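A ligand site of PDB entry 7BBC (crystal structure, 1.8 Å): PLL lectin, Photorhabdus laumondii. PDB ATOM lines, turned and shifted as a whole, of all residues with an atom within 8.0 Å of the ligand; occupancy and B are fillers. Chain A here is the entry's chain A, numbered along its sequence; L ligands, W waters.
O of Val 72 lies within hydrogen-bond range of O3 of the ligand (2.7 Å). N of Thr 94 is in hydrogen-bond range of O3 of the ligand (2.8 Å). OG1 of Thr 94 lies within hydrogen-bond range of O2 of the ligand, 2.7 Å away.
O of Gly 93 sits at hydrogen-bond distance from OG1 of Thr 74 (2.8 Å). NE1 of Trp 99 lies within hydrogen-bond range of OD1 of Asp 95 (3.0 Å). N of Trp 99 sits at hydrogen-bond distance from O of Val 91 (2.9 Å). The indole nitrogen (NE1) of Trp 114 sits close to the backbone carbonyl oxygen (O) of Asn 70, 3.2 Å away.
Residues that only touch the ligand: Gly 93 (3.2 Å), Gly 71 (3.6 Å), Trp 99 (3.6 Å) and Trp 114 (3.9 Å). Hydrophobic or aromatic side chains within 4 Å of the ligand: Trp 99 and Trp 114. Within 4 Å of the ligand: Gly 71, Val 72, Gly 93, Thr 94, Trp 99 and Trp 114.
Water W1 lies within hydrogen-bond range of an oxygen (O5) of the ligand (2.4 Å) and the backbone NH of Val 72 (3.1 Å). Water W2 bridges an oxygen (O2) of the ligand and the side-chain carboxylate (OD2) of Asp 95.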
ATOM      1  N   SER A  47     -31.151  20.501  11.194  1.00  0.00           N
ATOM      2  CA  SER A  47     -29.931  20.169  10.458  1.00  0.00           C
ATOM      3  C   SER A  47     -29.511  18.719  10.630  1.00  0.00           C
ATOM      4  O   SER A  47     -28.334  18.399  10.458  1.00  0.00           O
ATOM      5  CB  SER A  47     -28.791  21.098  10.844  1.00  0.00           C
ATOM      6  OG  SER A  47     -29.052  22.367  10.312  1.00  0.00           O
ATOM      7  N   VAL A  49     -30.343  14.568   9.528  1.00  0.00           N
ATOM      8  CA  VAL A  49     -30.963  13.713   8.504  1.00  0.00           C
ATOM      9  C   VAL A  49     -32.105  12.927   9.112  1.00  0.00           C
ATOM     10  O   VAL A  49     -31.948  12.248  10.134  1.00  0.00           O
ATOM     11  CB  VAL A  49     -29.933  12.749   7.896  1.00  0.00           C
ATOM     12  CG1 VAL A  49     -30.609  11.746   6.919  1.00  0.00           C
ATOM     13  CG2 VAL A  49     -28.852  13.517   7.181  1.00  0.00           C
ATOM     14  N   PHE A  69     -31.903  10.479  12.434  1.00  0.00           N
ATOM     15  CA  PHE A  69     -30.554  10.098  12.759  1.00  0.00           C
ATOM     16  C   PHE A  69     -29.921  11.211  13.605  1.00  0.00           C
ATOM     17  O   PHE A  69     -29.887  12.366  13.177  1.00  0.00           O
ATOM     18  CB  PHE A  69     -29.687   9.924  11.509  1.00  0.00           C
ATOM     19  CG  PHE A  69     -30.086   8.793  10.573  1.00  0.00           C
ATOM     20  CD1 PHE A  69     -30.488   7.562  11.053  1.00  0.00           C
ATOM     21  CD2 PHE A  69     -29.958   8.954   9.210  1.00  0.00           C
ATOM     22  CE1 PHE A  69     -30.784   6.543  10.187  1.00  0.00           C
ATOM     23  CE2 PHE A  69     -30.282   7.948   8.354  1.00  0.00           C
ATOM     24  CZ  PHE A  69     -30.691   6.750   8.833  1.00  0.00           C
ATOM     25  N   ASN A  70     -29.339  10.875  14.729  1.00  0.00           N
ATOM     26  CA  ASN A  70     -28.721  11.925  15.541  1.00  0.00           C
ATOM     27  C   ASN A  70     -27.450  12.423  14.869  1.00  0.00           C
ATOM     28  O   ASN A  70     -26.684  11.632  14.335  1.00  0.00           O
ATOM     29  CB  ASN A  70     -28.411  11.403  16.941  1.00  0.00           C
ATOM     30  CG  ASN A  70     -29.661  11.312  17.814  1.00  0.00           C
ATOM     31  OD1 ASN A  70     -30.538  12.177  17.757  1.00  0.00           O
ATOM     32  ND2 ASN A  70     -29.749  10.260  18.599  1.00  0.00           N
ATOM     33  N   GLY A  71     -27.263  13.725  14.818  1.00  0.00           N
ATOM     34  CA  GLY A  71     -26.043  14.318  14.311  1.00  0.00           C
ATOM     35  C   GLY A  71     -26.363  15.457  13.354  1.00  0.00           C
ATOM     36  O   GLY A  71     -27.339  15.362  12.616  1.00  0.00           O
ATOM     37  N   VAL A  72     -25.595  16.524  13.405  1.00  0.00           N
ATOM     38  CA  VAL A  72     -25.780  17.687  12.563  1.00  0.00           C
ATOM     39  C   VAL A  72     -24.936  17.485  11.311  1.00  0.00           C
ATOM     40  O   VAL A  72     -23.781  17.061  11.381  1.00  0.00           O
ATOM     41  CB  VAL A  72     -25.379  18.974  13.318  1.00  0.00           C
ATOM     42  CG1 VAL A  72     -25.403  20.179  12.397  1.00  0.00           C
ATOM     43  CG2 VAL A  72     -26.327  19.170  14.485  1.00  0.00           C
ATOM     44  N   VAL A  73     -25.511  17.836  10.168  1.00  0.00           N
ATOM     45  CA  VAL A  73     -24.890  17.598   8.872  1.00  0.00           C
ATOM     46  C   VAL A  73     -24.862  18.903   8.115  1.00  0.00           C
ATOM     47  O   VAL A  73     -25.596  19.845   8.429  1.00  0.00           O
ATOM     48  CB  VAL A  73     -25.604  16.486   8.033  1.00  0.00           C
ATOM     49  CG1 VAL A  73     -25.705  15.218   8.817  1.00  0.00           C
ATOM     50  CG2 VAL A  73     -27.014  16.917   7.492  1.00  0.00           C
ATOM     51  N   THR A  74     -23.978  18.957   7.124  1.00  0.00           N
ATOM     52  CA  THR A  74     -23.776  20.163   6.355  1.00  0.00           C
ATOM     53  C   THR A  74     -23.797  19.933   4.856  1.00  0.00           C
ATOM     54  O   THR A  74     -23.238  20.742   4.111  1.00  0.00           O
ATOM     55  CB  THR A  74     -22.453  20.829   6.713  1.00  0.00           C
ATOM     56  OG1 THR A  74     -21.380  19.921   6.417  1.00  0.00           O
ATOM     57  CG2 THR A  74     -22.413  21.208   8.184  1.00  0.00           C
ATOM     58  N   VAL A  91     -22.676  11.786   4.038  1.00  0.00           N
ATOM     59  CA  VAL A  91     -23.041  13.187   4.265  1.00  0.00           C
ATOM     60  C   VAL A  91     -21.820  13.910   4.810  1.00  0.00           C
ATOM     61  O   VAL A  91     -20.968  13.313   5.475  1.00  0.00           O
ATOM     62  CB  VAL A  91     -24.247  13.273   5.239  1.00  0.00           C
ATOM     63  CG1 VAL A  91     -23.811  13.124   6.690  1.00  0.00           C
ATOM     64  CG2 VAL A  91     -24.989  14.540   5.059  1.00  0.00           C
ATOM     65  N   ARG A  92     -21.735  15.209   4.527  1.00  0.00           N
ATOM     66  CA  ARG A  92     -20.694  16.050   5.091  1.00  0.00           C
ATOM     67  C   ARG A  92     -21.090  16.418   6.520  1.00  0.00           C
ATOM     68  O   ARG A  92     -22.267  16.693   6.796  1.00  0.00           O
ATOM     69  CB  ARG A  92     -20.477  17.293   4.243  1.00  0.00           C
ATOM     70  CG  ARG A  92     -19.170  18.039   4.627  1.00  0.00           C
ATOM     71  CD  ARG A  92     -18.869  19.264   3.755  1.00  0.00           C
ATOM     72  NE  ARG A  92     -19.836  20.345   3.947  1.00  0.00           N
ATOM     73  CZ  ARG A  92     -19.726  21.549   3.431  1.00  0.00           C
ATOM     74  NH1 ARG A  92     -18.691  21.866   2.678  1.00  0.00           N
ATOM     75  NH2 ARG A  92     -20.673  22.441   3.662  1.00  0.00           N
ATOM     76  N   GLY A  93     -20.107  16.401   7.417  1.00  0.00           N
ATOM     77  CA  GLY A  93     -20.331  16.716   8.814  1.00  0.00           C
ATOM     78  C   GLY A  93     -19.969  18.158   9.153  1.00  0.00           C
ATOM     79  O   GLY A  93     -19.561  18.942   8.308  1.00  0.00           O
ATOM     80  N   THR A  94     -20.190  18.512  10.422  1.00  0.00           N
ATOM     81  CA  THR A  94     -19.840  19.848  10.916  1.00  0.00           C
ATOM     82  C   THR A  94     -18.353  20.148  10.809  1.00  0.00           C
ATOM     83  O   THR A  94     -17.991  21.327  10.802  1.00  0.00           O
ATOM     84  CB  THR A  94     -20.281  20.018  12.375  1.00  0.00           C
ATOM     85  OG1 THR A  94     -19.717  18.987  13.189  1.00  0.00           O
ATOM     86  CG2 THR A  94     -21.761  19.905  12.477  1.00  0.00           C
ATOM     87  N   ASP A  95     -17.521  19.130  10.708  1.00  0.00           N
ATOM     88  CA  ASP A  95     -16.085  19.285  10.542  1.00  0.00           C
ATOM     89  C   ASP A  95     -15.652  19.302   9.092  1.00  0.00           C
ATOM     90  O   ASP A  95     -14.451  19.273   8.814  1.00  0.00           O
ATOM     91  CB  ASP A  95     -15.343  18.184  11.265  1.00  0.00           C
ATOM     92  CG  ASP A  95     -15.815  16.780  10.887  1.00  0.00           C
ATOM     93  OD1 ASP A  95     -16.657  16.611   9.971  1.00  0.00           O
ATOM     94  OD2 ASP A  95     -15.331  15.826  11.517  1.00  0.00           O
ATOM     95  N   ASN A  96     -16.611  19.380   8.185  1.00  0.00           N
ATOM     96  CA  ASN A  96     -16.397  19.355   6.752  1.00  0.00           C
ATOM     97  C   ASN A  96     -15.791  18.063   6.246  1.00  0.00           C
ATOM     98  O   ASN A  96     -15.335  17.998   5.086  1.00  0.00           O
ATOM     99  CB  ASN A  96     -15.568  20.565   6.329  1.00  0.00           C
ATOM    100  CG  ASN A  96     -16.406  21.834   6.341  1.00  0.00           C
ATOM    101  OD1 ASN A  96     -17.610  21.796   6.147  1.00  0.00           O
ATOM    102  ND2 ASN A  96     -15.776  22.938   6.646  1.00  0.00           N
ATOM    103  N   ALA A  97     -15.840  17.020   7.056  1.00  0.00           N
ATOM    104  CA  ALA A  97     -15.380  15.712   6.632  1.00  0.00           C
ATOM    105  C   ALA A  97     -16.568  14.868   6.184  1.00  0.00           C
ATOM    106  O   ALA A  97     -17.737  15.224   6.375  1.00  0.00           O
ATOM    107  CB  ALA A  97     -14.617  15.023   7.758  1.00  0.00           C
ATOM    108  N   LEU A  98     -16.242  13.730   5.613  1.00  0.00           N
ATOM    109  CA  LEU A  98     -17.227  12.760   5.160  1.00  0.00           C
ATOM    110  C   LEU A  98     -17.578  11.781   6.268  1.00  0.00           C
ATOM    111  O   LEU A  98     -16.681  11.231   6.925  1.00  0.00           O
ATOM    112  CB  LEU A  98     -16.703  12.000   3.947  1.00  0.00           C
ATOM    113  CG  LEU A  98     -17.717  11.074   3.237  1.00  0.00           C
ATOM    114  CD1 LEU A  98     -18.768  11.871   2.565  1.00  0.00           C
ATOM    115  CD2 LEU A  98     -16.974  10.137   2.223  1.00  0.00           C
ATOM    116  N   TRP A  99     -18.874  11.582   6.475  1.00  0.00           N
ATOM    117  CA  TRP A  99     -19.403  10.633   7.441  1.00  0.00           C
ATOM    118  C   TRP A  99     -20.350   9.654   6.733  1.00  0.00           C
ATOM    119  O   TRP A  99     -20.917   9.972   5.675  1.00  0.00           O
ATOM    120  CB  TRP A  99     -20.142  11.358   8.556  1.00  0.00           C
ATOM    121  CG  TRP A  99     -19.193  12.210   9.409  1.00  0.00           C
ATOM    122  CD1 TRP A  99     -18.635  13.392   9.072  1.00  0.00           C
ATOM    123  CD2 TRP A  99     -18.724  11.909  10.727  1.00  0.00           C
ATOM    124  NE1 TRP A  99     -17.839  13.867  10.091  1.00  0.00           N
ATOM    125  CE2 TRP A  99     -17.862  12.957  11.112  1.00  0.00           C
ATOM    126  CE3 TRP A  99     -18.944  10.857  11.606  1.00  0.00           C
ATOM    127  CZ2 TRP A  99     -17.263  12.995  12.355  1.00  0.00           C
ATOM    128  CZ3 TRP A  99     -18.334  10.870  12.818  1.00  0.00           C
ATOM    129  CH2 TRP A  99     -17.494  11.934  13.192  1.00  0.00           C
ATOM    130  N   HIS A 100     -20.489   8.465   7.292  1.00  0.00           N
ATOM    131  CA  HIS A 100     -21.439   7.517   6.721  1.00  0.00           C
ATOM    132  C   HIS A 100     -22.122   6.703   7.800  1.00  0.00           C
ATOM    133  O   HIS A 100     -21.625   6.570   8.913  1.00  0.00           O
ATOM    134  CB  HIS A 100     -20.790   6.563   5.670  1.00  0.00           C
ATOM    135  CG  HIS A 100     -19.712   5.668   6.161  1.00  0.00           C
ATOM    136  ND1 HIS A 100     -19.571   4.368   5.705  1.00  0.00           N
ATOM    137  CD2 HIS A 100     -18.685   5.883   7.015  1.00  0.00           C
ATOM    138  CE1 HIS A 100     -18.528   3.800   6.291  1.00  0.00           C
ATOM    139  NE2 HIS A 100     -17.963   4.710   7.077  1.00  0.00           N
ATOM    140  N   SER A 113     -25.204   4.389  13.044  1.00  0.00           N
ATOM    141  CA  SER A 113     -24.904   5.741  13.500  1.00  0.00           C
ATOM    142  C   SER A 113     -23.703   6.247  12.708  1.00  0.00           C
ATOM    143  O   SER A 113     -23.056   5.478  11.984  1.00  0.00           O
ATOM    144  CB  SER A 113     -24.644   5.835  15.014  1.00  0.00           C
ATOM    145  OG  SER A 113     -23.335   5.390  15.373  1.00  0.00           O
ATOM    146  N   TRP A 114     -23.410   7.530  12.797  1.00  0.00           N
ATOM    147  CA  TRP A 114     -22.488   8.129  11.850  1.00  0.00           C
ATOM    148  C   TRP A 114     -21.064   7.756  12.223  1.00  0.00           C
ATOM    149  O   TRP A 114     -20.655   7.879  13.373  1.00  0.00           O
ATOM    150  CB  TRP A 114     -22.600   9.647  11.840  1.00  0.00           C
ATOM    151  CG  TRP A 114     -23.906  10.199  11.329  1.00  0.00           C
ATOM    152  CD1 TRP A 114     -24.865  10.853  12.061  1.00  0.00           C
ATOM    153  CD2 TRP A 114     -24.396  10.132  10.001  1.00  0.00           C
ATOM    154  NE1 TRP A 114     -25.887  11.214  11.275  1.00  0.00           N
ATOM    155  CE2 TRP A 114     -25.647  10.777   9.991  1.00  0.00           C
ATOM    156  CE3 TRP A 114     -23.913   9.612   8.808  1.00  0.00           C
ATOM    157  CZ2 TRP A 114     -26.422  10.899   8.852  1.00  0.00           C
ATOM    158  CZ3 TRP A 114     -24.676   9.743   7.669  1.00  0.00           C
ATOM    159  CH2 TRP A 114     -25.919  10.377   7.697  1.00  0.00           C
ATOM    160  N   GLN A 115     -20.287   7.358  11.241  1.00  0.00           N
ATOM    161  CA  GLN A 115     -18.899   6.969  11.438  1.00  0.00           C
ATOM    162  C   GLN A 115     -18.026   7.748  10.465  1.00  0.00           C
ATOM    163  O   GLN A 115     -18.460   8.077   9.359  1.00  0.00           O
ATOM    164  CB  GLN A 115     -18.700   5.470  11.169  1.00  0.00           C
ATOM    165  CG  GLN A 115     -19.612   4.564  11.957  1.00  0.00           C
ATOM    166  CD  GLN A 115     -19.406   4.587  13.411  1.00  0.00           C
ATOM    167  OE1 GLN A 115     -20.361   4.445  14.203  1.00  0.00           O
ATOM    168  NE2 GLN A 115     -18.179   4.739  13.811  1.00  0.00           N
ATOM    169  N   PRO A 116     -16.789   8.038  10.847  1.00  0.00           N
ATOM    170  CA  PRO A 116     -15.996   8.984  10.065  1.00  0.00           C
ATOM    171  C   PRO A 116     -15.235   8.334   8.923  1.00  0.00           C
ATOM    172  O   PRO A 116     -14.620   7.280   9.083  1.00  0.00           O
ATOM    173  CB  PRO A 116     -14.991   9.534  11.100  1.00  0.00           C
ATOM    174  CG  PRO A 116     -14.830   8.442  12.062  1.00  0.00           C
ATOM    175  CD  PRO A 116     -16.195   7.795  12.185  1.00  0.00           C
HETATM  176  C1  LIG L   1     -21.807  14.193  14.668  1.00  0.00           C
HETATM  177  C2  LIG L   1     -20.911  15.430  14.661  1.00  0.00           C
HETATM  178  O1  LIG L   1     -20.246  15.628  15.932  1.00  0.00           O
HETATM  179  C3  LIG L   1     -19.941  15.230  13.540  1.00  0.00           C
HETATM  180  O2  LIG L   1     -19.040  16.364  13.389  1.00  0.00           O
HETATM  181  C4  LIG L   1     -20.636  15.034  12.192  1.00  0.00           C
HETATM  182  O3  LIG L   1     -21.263  16.274  11.820  1.00  0.00           O
HETATM  183  C5  LIG L   1     -21.673  13.912  12.251  1.00  0.00           C
HETATM  184  C6  LIG L   1     -22.577  13.829  11.054  1.00  0.00           C
HETATM  185  O4  LIG L   1     -22.566  14.129  13.380  1.00  0.00           O
HETATM  186  O5  LIG L   1     -22.719  14.245  15.672  1.00  0.00           O
HETATM  187  O   HOH W   1     -23.643  16.502  15.832  1.00  0.00           O
HETATM  188  O   HOH W   2     -16.612  16.003  14.567  1.00  0.00           O
